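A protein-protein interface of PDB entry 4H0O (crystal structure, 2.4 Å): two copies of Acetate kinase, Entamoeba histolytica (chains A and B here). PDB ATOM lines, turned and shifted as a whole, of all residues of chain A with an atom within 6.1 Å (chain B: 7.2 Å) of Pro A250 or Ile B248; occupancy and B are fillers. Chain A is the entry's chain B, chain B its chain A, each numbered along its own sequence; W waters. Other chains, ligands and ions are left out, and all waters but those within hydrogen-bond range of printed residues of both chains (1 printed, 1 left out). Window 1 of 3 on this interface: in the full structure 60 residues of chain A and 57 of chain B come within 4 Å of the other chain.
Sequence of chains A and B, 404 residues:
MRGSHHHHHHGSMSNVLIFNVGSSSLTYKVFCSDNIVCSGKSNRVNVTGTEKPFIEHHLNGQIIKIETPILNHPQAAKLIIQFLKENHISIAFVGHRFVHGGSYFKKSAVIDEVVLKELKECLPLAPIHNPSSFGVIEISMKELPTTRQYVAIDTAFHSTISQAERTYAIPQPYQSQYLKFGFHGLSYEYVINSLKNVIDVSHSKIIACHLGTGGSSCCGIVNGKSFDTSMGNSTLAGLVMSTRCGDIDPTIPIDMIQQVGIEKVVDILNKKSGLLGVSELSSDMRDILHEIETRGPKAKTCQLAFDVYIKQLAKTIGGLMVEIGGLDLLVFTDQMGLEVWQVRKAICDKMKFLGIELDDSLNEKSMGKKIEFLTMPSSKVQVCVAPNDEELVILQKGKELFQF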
ATOM      1  N   TYR A 168      -5.576  -8.175  24.620  1.00  0.00           N
ATOM      2  CA  TYR A 168      -6.843  -7.456  24.607  1.00  0.00           C
ATOM      3  C   TYR A 168      -7.238  -7.048  26.027  1.00  0.00           C
ATOM      4  O   TYR A 168      -6.994  -7.783  26.986  1.00  0.00           O
ATOM      5  CB  TYR A 168      -7.936  -8.308  23.961  1.00  0.00           C
ATOM      6  CG  TYR A 168      -7.726  -8.528  22.482  1.00  0.00           C
ATOM      7  CD1 TYR A 168      -7.917  -7.492  21.576  1.00  0.00           C
ATOM      8  CD2 TYR A 168      -7.341  -9.769  21.988  1.00  0.00           C
ATOM      9  CE1 TYR A 168      -7.728  -7.681  20.224  1.00  0.00           C
ATOM     10  CE2 TYR A 168      -7.149  -9.969  20.631  1.00  0.00           C
ATOM     11  CZ  TYR A 168      -7.345  -8.919  19.755  1.00  0.00           C
ATOM     12  OH  TYR A 168      -7.160  -9.101  18.405  1.00  0.00           O
ATOM     13  N   ALA A 169      -7.854  -5.878  26.156  1.00  0.00           N
ATOM     14  CA  ALA A 169      -8.192  -5.329  27.466  1.00  0.00           C
ATOM     15  C   ALA A 169      -9.346  -6.073  28.150  1.00  0.00           C
ATOM     16  O   ALA A 169     -10.368  -5.467  28.483  1.00  0.00           O
ATOM     17  CB  ALA A 169      -8.512  -3.846  27.348  1.00  0.00           C
ATOM     18  N   ILE A 170      -9.160  -7.376  28.370  1.00  0.00           N
ATOM     19  CA  ILE A 170     -10.138  -8.228  29.049  1.00  0.00           C
ATOM     20  C   ILE A 170      -9.483  -8.931  30.249  1.00  0.00           C
ATOM     21  O   ILE A 170      -8.259  -9.052  30.303  1.00  0.00           O
ATOM     22  CB  ILE A 170     -10.732  -9.283  28.081  1.00  0.00           C
ATOM     23  CG1 ILE A 170      -9.621 -10.109  27.430  1.00  0.00           C
ATOM     24  CG2 ILE A 170     -11.601  -8.614  27.021  1.00  0.00           C
ATOM     25  CD1 ILE A 170     -10.129 -11.304  26.638  1.00  0.00           C
ATOM     26  N   ALA A 237     -10.432 -10.694  12.229  1.00  0.00           N
ATOM     27  CA  ALA A 237     -10.164  -9.335  12.697  1.00  0.00           C
ATOM     28  C   ALA A 237      -9.377  -8.485  11.695  1.00  0.00           C
ATOM     29  O   ALA A 237      -8.655  -9.012  10.842  1.00  0.00           O
ATOM     30  CB  ALA A 237      -9.435  -9.381  14.026  1.00  0.00           C
ATOM     31  N   ASP A 247     -12.597  -5.647  11.831  1.00  0.00           N
ATOM     32  CA  ASP A 247     -12.933  -5.037  13.117  1.00  0.00           C
ATOM     33  C   ASP A 247     -14.294  -4.335  13.099  1.00  0.00           C
ATOM     34  O   ASP A 247     -14.522  -3.417  12.309  1.00  0.00           O
ATOM     35  CB  ASP A 247     -11.849  -4.046  13.550  1.00  0.00           C
ATOM     36  CG  ASP A 247     -10.579  -4.731  14.033  1.00  0.00           C
ATOM     37  OD1 ASP A 247     -10.635  -5.919  14.422  1.00  0.00           O
ATOM     38  OD2 ASP A 247      -9.520  -4.068  14.035  1.00  0.00           O
ATOM     39  N   ILE A 248     -15.193  -4.777  13.974  1.00  0.00           N
ATOM     40  CA  ILE A 248     -16.499  -4.142  14.138  1.00  0.00           C
ATOM     41  C   ILE A 248     -16.804  -3.957  15.622  1.00  0.00           C
ATOM     42  O   ILE A 248     -16.080  -4.477  16.474  1.00  0.00           O
ATOM     43  CB  ILE A 248     -17.622  -4.983  13.503  1.00  0.00           C
ATOM     44  CG1 ILE A 248     -17.641  -6.384  14.115  1.00  0.00           C
ATOM     45  CG2 ILE A 248     -17.458  -5.051  11.982  1.00  0.00           C
ATOM     46  CD1 ILE A 248     -18.788  -7.253  13.620  1.00  0.00           C
ATOM     47  N   ASP A 249     -17.869  -3.219  15.926  1.00  0.00           N
ATOM     48  CA  ASP A 249     -18.328  -3.045  17.302  1.00  0.00           C
ATOM     49  C   ASP A 249     -18.558  -4.414  17.952  1.00  0.00           C
ATOM     50  O   ASP A 249     -19.363  -5.208  17.466  1.00  0.00           O
ATOM     51  CB  ASP A 249     -19.620  -2.221  17.313  1.00  0.00           C
ATOM     52  CG  ASP A 249     -19.988  -1.708  18.698  1.00  0.00           C
ATOM     53  OD1 ASP A 249     -19.829  -2.453  19.690  1.00  0.00           O
ATOM     54  OD2 ASP A 249     -20.454  -0.549  18.790  1.00  0.00           O
ATOM     55  N   PRO A 250     -17.835  -4.696  19.049  1.00  0.00           N
ATOM     56  CA  PRO A 250     -17.858  -5.988  19.753  1.00  0.00           C
ATOM     57  C   PRO A 250     -19.249  -6.393  20.241  1.00  0.00           C
ATOM     58  O   PRO A 250     -19.489  -7.576  20.498  1.00  0.00           O
ATOM     59  CB  PRO A 250     -16.940  -5.746  20.957  1.00  0.00           C
ATOM     60  CG  PRO A 250     -16.033  -4.645  20.529  1.00  0.00           C
ATOM     61  CD  PRO A 250     -16.872  -3.757  19.650  1.00  0.00           C
ATOM     62  N   THR A 251     -20.146  -5.419  20.375  1.00  0.00           N
ATOM     63  CA  THR A 251     -21.513  -5.684  20.815  1.00  0.00           C
ATOM     64  C   THR A 251     -22.353  -6.271  19.671  1.00  0.00           C
ATOM     65  O   THR A 251     -23.326  -6.994  19.905  1.00  0.00           O
ATOM     66  CB  THR A 251     -22.174  -4.402  21.378  1.00  0.00           C
ATOM     67  OG1 THR A 251     -21.383  -3.886  22.459  1.00  0.00           O
ATOM     68  CG2 THR A 251     -23.575  -4.685  21.891  1.00  0.00           C
ATOM     69  N   ILE A 252     -21.960  -5.970  18.433  1.00  0.00           N
ATOM     70  CA  ILE A 252     -22.694  -6.448  17.259  1.00  0.00           C
ATOM     71  C   ILE A 252     -22.830  -7.979  17.162  1.00  0.00           C
ATOM     72  O   ILE A 252     -23.936  -8.473  16.935  1.00  0.00           O
ATOM     73  CB  ILE A 252     -22.148  -5.850  15.935  1.00  0.00           C
ATOM     74  CG1 ILE A 252     -22.260  -4.326  15.960  1.00  0.00           C
ATOM     75  CG2 ILE A 252     -22.913  -6.396  14.743  1.00  0.00           C
ATOM     76  CD1 ILE A 252     -21.831  -3.651  14.668  1.00  0.00           C
ATOM     77  N   PRO A 253     -21.721  -8.732  17.323  1.00  0.00           N
ATOM     78  CA  PRO A 253     -21.914 -10.187  17.279  1.00  0.00           C
ATOM     79  C   PRO A 253     -22.870 -10.653  18.373  1.00  0.00           C
ATOM     80  O   PRO A 253     -23.760 -11.446  18.080  1.00  0.00           O
ATOM     81  CB  PRO A 253     -20.508 -10.738  17.539  1.00  0.00           C
ATOM     82  CG  PRO A 253     -19.588  -9.650  17.115  1.00  0.00           C
ATOM     83  CD  PRO A 253     -20.296  -8.373  17.457  1.00  0.00           C
ATOM     84  N   ILE A 254     -22.695 -10.148  19.594  1.00  0.00           N
ATOM     85  CA  ILE A 254     -23.556 -10.493  20.726  1.00  0.00           C
ATOM     86  C   ILE A 254     -25.048 -10.300  20.417  1.00  0.00           C
ATOM     87  O   ILE A 254     -25.866 -11.184  20.684  1.00  0.00           O
ATOM     88  CB  ILE A 254     -23.190  -9.669  21.982  1.00  0.00           C
ATOM     89  CG1 ILE A 254     -21.700  -9.816  22.313  1.00  0.00           C
ATOM     90  CG2 ILE A 254     -24.050 -10.079  23.169  1.00  0.00           C
ATOM     91  CD1 ILE A 254     -21.233  -8.952  23.479  1.00  0.00           C
ATOM     92  N   TYR B 168     -20.613  -0.535   9.175  1.00  0.00           N
ATOM     93  CA  TYR B 168     -19.751  -1.696   9.362  1.00  0.00           C
ATOM     94  C   TYR B 168     -19.874  -2.653   8.171  1.00  0.00           C
ATOM     95  O   TYR B 168     -20.944  -2.789   7.575  1.00  0.00           O
ATOM     96  CB  TYR B 168     -20.097  -2.411  10.664  1.00  0.00           C
ATOM     97  CG  TYR B 168     -19.768  -1.599  11.888  1.00  0.00           C
ATOM     98  CD1 TYR B 168     -18.467  -1.530  12.362  1.00  0.00           C
ATOM     99  CD2 TYR B 168     -20.755  -0.900  12.571  1.00  0.00           C
ATOM    100  CE1 TYR B 168     -18.156  -0.789  13.481  1.00  0.00           C
ATOM    101  CE2 TYR B 168     -20.454  -0.156  13.692  1.00  0.00           C
ATOM    102  CZ  TYR B 168     -19.152  -0.106  14.143  1.00  0.00           C
ATOM    103  OH  TYR B 168     -18.836   0.632  15.257  1.00  0.00           O
ATOM    104  N   SER B 234     -22.620   0.792  19.984  1.00  0.00           N
ATOM    105  CA  SER B 234     -22.695   0.718  21.440  1.00  0.00           C
ATOM    106  C   SER B 234     -21.594   1.556  22.090  1.00  0.00           C
ATOM    107  O   SER B 234     -20.691   2.052  21.411  1.00  0.00           O
ATOM    108  CB  SER B 234     -22.584  -0.735  21.903  1.00  0.00           C
ATOM    109  OG  SER B 234     -21.272  -1.238  21.718  1.00  0.00           O
ATOM    110  N   LEU B 236     -19.422   0.409  24.053  1.00  0.00           N
ATOM    111  CA  LEU B 236     -18.372  -0.545  24.394  1.00  0.00           C
ATOM    112  C   LEU B 236     -17.190  -0.396  23.434  1.00  0.00           C
ATOM    113  O   LEU B 236     -16.052  -0.711  23.776  1.00  0.00           O
ATOM    114  CB  LEU B 236     -18.928  -1.972  24.320  1.00  0.00           C
ATOM    115  CG  LEU B 236     -18.012  -3.138  24.699  1.00  0.00           C
ATOM    116  CD1 LEU B 236     -17.547  -2.969  26.125  1.00  0.00           C
ATOM    117  CD2 LEU B 236     -18.709  -4.481  24.535  1.00  0.00           C
ATOM    118  N   ALA B 237     -17.474   0.103  22.235  1.00  0.00           N
ATOM    119  CA  ALA B 237     -16.497   0.149  21.146  1.00  0.00           C
ATOM    120  C   ALA B 237     -15.395   1.196  21.332  1.00  0.00           C
ATOM    121  O   ALA B 237     -15.592   2.212  22.003  1.00  0.00           O
ATOM    122  CB  ALA B 237     -17.214   0.385  19.824  1.00  0.00           C
ATOM    123  N   GLY B 238     -14.238   0.942  20.723  1.00  0.00           N
ATOM    124  CA  GLY B 238     -13.186   1.939  20.629  1.00  0.00           C
ATOM    125  C   GLY B 238     -12.027   1.805  21.601  1.00  0.00           C
ATOM    126  O   GLY B 238     -11.294   0.813  21.592  1.00  0.00           O
ATOM    127  N   CYS B 245     -13.829  -3.038  27.506  1.00  0.00           N
ATOM    128  CA  CYS B 245     -12.754  -3.609  26.702  1.00  0.00           C
ATOM    129  C   CYS B 245     -12.334  -2.754  25.506  1.00  0.00           C
ATOM    130  O   CYS B 245     -11.167  -2.772  25.108  1.00  0.00           O
ATOM    131  CB  CYS B 245     -13.155  -4.999  26.215  1.00  0.00           C
ATOM    132  SG  CYS B 245     -14.625  -5.003  25.174  1.00  0.00           S
ATOM    133  N   GLY B 246     -13.277  -2.014  24.933  1.00  0.00           N
ATOM    134  CA  GLY B 246     -13.006  -1.275  23.711  1.00  0.00           C
ATOM    135  C   GLY B 246     -12.990  -2.224  22.524  1.00  0.00           C
ATOM    136  O   GLY B 246     -13.496  -3.347  22.619  1.00  0.00           O
ATOM    137  N   ASP B 247     -12.414  -1.783  21.409  1.00  0.00           N
ATOM    138  CA  ASP B 247     -12.323  -2.630  20.224  1.00  0.00           C
ATOM    139  C   ASP B 247     -11.479  -3.888  20.476  1.00  0.00           C
ATOM    140  O   ASP B 247     -10.320  -3.803  20.882  1.00  0.00           O
ATOM    141  CB  ASP B 247     -11.771  -1.839  19.030  1.00  0.00           C
ATOM    142  CG  ASP B 247     -12.770  -0.817  18.484  1.00  0.00           C
ATOM    143  OD1 ASP B 247     -13.988  -0.957  18.734  1.00  0.00           O
ATOM    144  OD2 ASP B 247     -12.332   0.126  17.791  1.00  0.00           O
ATOM    145  N   ILE B 248     -12.082  -5.052  20.249  1.00  0.00           N
ATOM    146  CA  ILE B 248     -11.393  -6.334  20.374  1.00  0.00           C
ATOM    147  C   ILE B 248     -11.740  -7.236  19.195  1.00  0.00           C
ATOM    148  O   ILE B 248     -12.637  -6.920  18.408  1.00  0.00           O
ATOM    149  CB  ILE B 248     -11.794  -7.074  21.662  1.00  0.00           C
ATOM    150  CG1 ILE B 248     -13.307  -7.297  21.689  1.00  0.00           C
ATOM    151  CG2 ILE B 248     -11.314  -6.322  22.906  1.00  0.00           C
ATOM    152  CD1 ILE B 248     -13.787  -8.101  22.879  1.00  0.00           C
ATOM    153  N   ASP B 249     -11.035  -8.359  19.081  1.00  0.00           N
ATOM    154  CA  ASP B 249     -11.331  -9.366  18.064  1.00  0.00           C
ATOM    155  C   ASP B 249     -12.779  -9.839  18.229  1.00  0.00           C
ATOM    156  O   ASP B 249     -13.151 -10.346  19.290  1.00  0.00           O
ATOM    157  CB  ASP B 249     -10.359 -10.540  18.206  1.00  0.00           C
ATOM    158  CG  ASP B 249     -10.346 -11.455  16.994  1.00  0.00           C
ATOM    159  OD1 ASP B 249     -11.389 -11.595  16.320  1.00  0.00           O
ATOM    160  OD2 ASP B 249      -9.282 -12.050  16.719  1.00  0.00           O
ATOM    161  N   PRO B 250     -13.604  -9.652  17.185  1.00  0.00           N
ATOM    162  CA  PRO B 250     -15.047  -9.937  17.216  1.00  0.00           C
ATOM    163  C   PRO B 250     -15.420 -11.396  17.491  1.00  0.00           C
ATOM    164  O   PRO B 250     -16.556 -11.649  17.888  1.00  0.00           O
ATOM    165  CB  PRO B 250     -15.511  -9.551  15.807  1.00  0.00           C
ATOM    166  CG  PRO B 250     -14.499  -8.574  15.324  1.00  0.00           C
ATOM    167  CD  PRO B 250     -13.194  -9.014  15.921  1.00  0.00           C
ATOM    168  N   THR B 251     -14.504 -12.335  17.272  1.00  0.00           N
ATOM    169  CA  THR B 251     -14.813 -13.743  17.528  1.00  0.00           C
ATOM    170  C   THR B 251     -14.712 -14.071  19.013  1.00  0.00           C
ATOM    171  O   THR B 251     -15.256 -15.075  19.471  1.00  0.00           O
ATOM    172  CB  THR B 251     -13.906 -14.700  16.724  1.00  0.00           C
ATOM    173  OG1 THR B 251     -12.568 -14.641  17.232  1.00  0.00           O
ATOM    174  CG2 THR B 251     -13.908 -14.321  15.258  1.00  0.00           C
ATOM    175  N   ILE B 252     -14.004 -13.220  19.751  1.00  0.00           N
ATOM    176  CA  ILE B 252     -13.843 -13.391  21.196  1.00  0.00           C
ATOM    177  C   ILE B 252     -15.165 -13.307  21.986  1.00  0.00           C
ATOM    178  O   ILE B 252     -15.422 -14.160  22.840  1.00  0.00           O
ATOM    179  CB  ILE B 252     -12.781 -12.415  21.782  1.00  0.00           C
ATOM    180  CG1 ILE B 252     -11.398 -12.722  21.208  1.00  0.00           C
ATOM    181  CG2 ILE B 252     -12.746 -12.495  23.300  1.00  0.00           C
ATOM    182  CD1 ILE B 252     -10.315 -11.737  21.642  1.00  0.00           C
ATOM    183  N   PRO B 253     -16.005 -12.284  21.718  1.00  0.00           N
ATOM    184  CA  PRO B 253     -17.305 -12.298  22.398  1.00  0.00           C
ATOM    185  C   PRO B 253     -18.088 -13.563  22.075  1.00  0.00           C
ATOM    186  O   PRO B 253     -18.831 -14.048  22.923  1.00  0.00           O
ATOM    187  CB  PRO B 253     -18.025 -11.087  21.800  1.00  0.00           C
ATOM    188  CG  PRO B 253     -16.939 -10.170  21.384  1.00  0.00           C
ATOM    189  CD  PRO B 253     -15.819 -11.055  20.924  1.00  0.00           C
ATOM    190  N   ILE B 254     -17.911 -14.091  20.865  1.00  0.00           N
ATOM    191  CA  ILE B 254     -18.609 -15.298  20.433  1.00  0.00           C
ATOM    192  C   ILE B 254     -18.091 -16.543  21.156  1.00  0.00           C
ATOM    193  O   ILE B 254     -18.879 -17.380  21.608  1.00  0.00           O
ATOM    194  CB  ILE B 254     -18.493 -15.490  18.910  1.00  0.00           C
ATOM    195  CG1 ILE B 254     -19.043 -14.261  18.184  1.00  0.00           C
ATOM    196  CG2 ILE B 254     -19.236 -16.739  18.466  1.00  0.00           C
ATOM    197  CD1 ILE B 254     -18.891 -14.304  16.676  1.00  0.00           C
ATOM    198  N   MET B 256     -16.499 -16.583  24.074  1.00  0.00           N
ATOM    199  CA  MET B 256     -16.831 -16.458  25.495  1.00  0.00           C
ATOM    200  C   MET B 256     -18.286 -16.843  25.769  1.00  0.00           C
ATOM    201  O   MET B 256     -18.598 -17.446  26.799  1.00  0.00           O
ATOM    202  CB  MET B 256     -16.553 -15.037  26.000  1.00  0.00           C
ATOM    203  CG  MET B 256     -15.073 -14.680  26.113  1.00  0.00           C
ATOM    204  SD  MET B 256     -14.787 -12.917  26.399  1.00  0.00           S
ATOM    205  CE  MET B 256     -15.650 -12.672  27.955  1.00  0.00           C
ATOM    206  N   VAL B 265     -21.238 -12.527  29.444  1.00  0.00           N
ATOM    207  CA  VAL B 265     -20.225 -11.929  28.576  1.00  0.00           C
ATOM    208  C   VAL B 265     -20.384 -10.411  28.532  1.00  0.00           C
ATOM    209  O   VAL B 265     -19.410  -9.673  28.689  1.00  0.00           O
ATOM    210  CB  VAL B 265     -20.303 -12.502  27.148  1.00  0.00           C
ATOM    211  CG1 VAL B 265     -19.543 -11.624  26.166  1.00  0.00           C
ATOM    212  CG2 VAL B 265     -19.766 -13.917  27.121  1.00  0.00           C
ATOM    213  N   LEU B 269     -17.480  -7.708  29.682  1.00  0.00           N
ATOM    214  CA  LEU B 269     -16.905  -6.762  28.728  1.00  0.00           C
ATOM    215  C   LEU B 269     -17.166  -5.306  29.117  1.00  0.00           C
ATOM    216  O   LEU B 269     -16.423  -4.411  28.706  1.00  0.00           O
ATOM    217  CB  LEU B 269     -17.426  -7.043  27.311  1.00  0.00           C
ATOM    218  CG  LEU B 269     -17.111  -8.429  26.737  1.00  0.00           C
ATOM    219  CD1 LEU B 269     -17.649  -8.592  25.323  1.00  0.00           C
ATOM    220  CD2 LEU B 269     -15.617  -8.684  26.761  1.00  0.00           C
ATOM    221  N   GLN B 312      -3.851   1.589  22.471  1.00  0.00           N
ATOM    222  CA  GLN B 312      -5.155   1.708  21.835  1.00  0.00           C
ATOM    223  C   GLN B 312      -5.530   3.168  21.595  1.00  0.00           C
ATOM    224  O   GLN B 312      -6.147   3.502  20.578  1.00  0.00           O
ATOM    225  CB  GLN B 312      -6.226   1.005  22.672  1.00  0.00           C
ATOM    226  CG  GLN B 312      -7.614   0.993  22.039  1.00  0.00           C
ATOM    227  CD  GLN B 312      -7.670   0.210  20.737  1.00  0.00           C
ATOM    228  OE1 GLN B 312      -6.748  -0.535  20.401  1.00  0.00           O
ATOM    229  NE2 GLN B 312      -8.763   0.374  19.998  1.00  0.00           N
HETATM  230  O   HOH W   1     -13.421  -4.522  17.121  1.00  0.00           O
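The side-chain carboxylate (OD1) of Asp B249 lies close to the backbone NH (N) of Thr B251.
O of Leu B269 sits at hydrogen-bond distance from N of Cys B245 (3.2 Å).
N of Thr A251 is in hydrogen-bond range of OD1 of Asp A249 (3.1 Å).
The side-chain hydroxyl (OG) of Ser B234 sits close to the backbone NH (N) of Leu B236 (3.4 Å).
The backbone NH of Gly B246 sits close to the backbone carbonyl oxygen of Leu B236.
Water W1 bridges the backbone carbonyl oxygen of Ile A248 (2.7 Å) and the backbone carbonyl oxygen of Ile B248 (2.8 Å).
Of the 12 printed residues of chain A, 10 touch a printed residue of chain B.
Printed residues of chain A that touch a printed residue of chain B: Tyr A168, Ala A169, Ala A237, Ile A248, Asp A249, Pro A250, Thr A251, Ile A252, Pro A253 and Ile A254.
Hydrophobic or aromatic side chains of chain A within 4 Å of the printed part of chain B: Tyr A168, Ala A169, Ala A237, Ile A248, Pro A250, Ile A252, Pro A253 and Ile A254.
Of the 19 printed residues of chain B, 12 touch a printed residue of chain A.
Hydrophobic or aromatic side chains of chain B within 4 Å of the printed part of chain A: Tyr B168, Leu B236, Ala B237, Ile B248, Ile B252, Pro B253 and Ile B254.
Among the printed residues, no Asp or Glu carboxylate lies within 4 Å of a Lys or Arg side-chain nitrogen of the other chain.
OG of Ser B234 is in hydrogen-bond range of OG1 of Thr A251, 2.8 Å away.
The side-chain hydroxyl (OG) of Ser B234 sits at hydrogen-bond distance from the side-chain carboxylate (OD1) of Asp A249 (2.8 Å).
Of the printed residues of chain B, Ala A237 touches Asp B249.
Pro A250 touches just these residues of chain B: Gly B246, Ile B248 and Pro B253.
Of the printed residues of chain B, Thr A251 touches Ser B234 (2.8 Å) and Leu B236 (3.4 Å).
Printed residues of chain B within 4 Å of Ile A252: Tyr B168 (3.6 Å).
Printed residues of chain A within 4 Å of Cys B245: Ala A169.
Of the printed residues of chain A, Ile B248 touches Tyr A168 and Pro A250.
Met B256 touches none of the printed residues of chain A.
The nearest residue of chain B that does not touch Pro A250 is Asp B247 (4.1 Å).
The nearest residue of chain A that does not touch Ile B248 is Asp A247 (4.6 Å).
Tyr A168 touches Ile B248, and with the chains exchanged Ile A248 touches Tyr B168.
Tyr A168 touches Ile B252, and with the chains exchanged Ile A252 touches Tyr B168.
Ala A237 touches Asp B249, and with the chains exchanged Asp A249 touches Ala B237.
Pro A253 touches Ile B254, and with the chains exchanged Ile A254 touches Pro B253.
Positions printed for both chains: 168, 237, 247, 248, 249, 250, 251, 252, 253 and 254.
Of the 18 pairs that touch across the chains among the printed residues, 12 have their exchanged pair printed and touching as well.
Tyr A168 touches Ile B248.
Ile B252 touches Tyr A168.
CB of Ala A237 touches CG of Asp B249, 3.7 Å away.
Asp A249 touches Ala B237.
Ile B248 touches Pro A250 (CG1 to CG, 3.98 Å).
O of Pro A250 touches CG of Pro B253, 3.7 Å away.
Leu B236 touches Thr A251 (CD2 to OG1, 3.4 Å).
Ile A252 touches Tyr B168 (CD1 to CD2, 3.6 Å).
O of Pro B250 touches CG of Pro A253, 3.7 Å away.
Ile A254 touches Pro B253.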
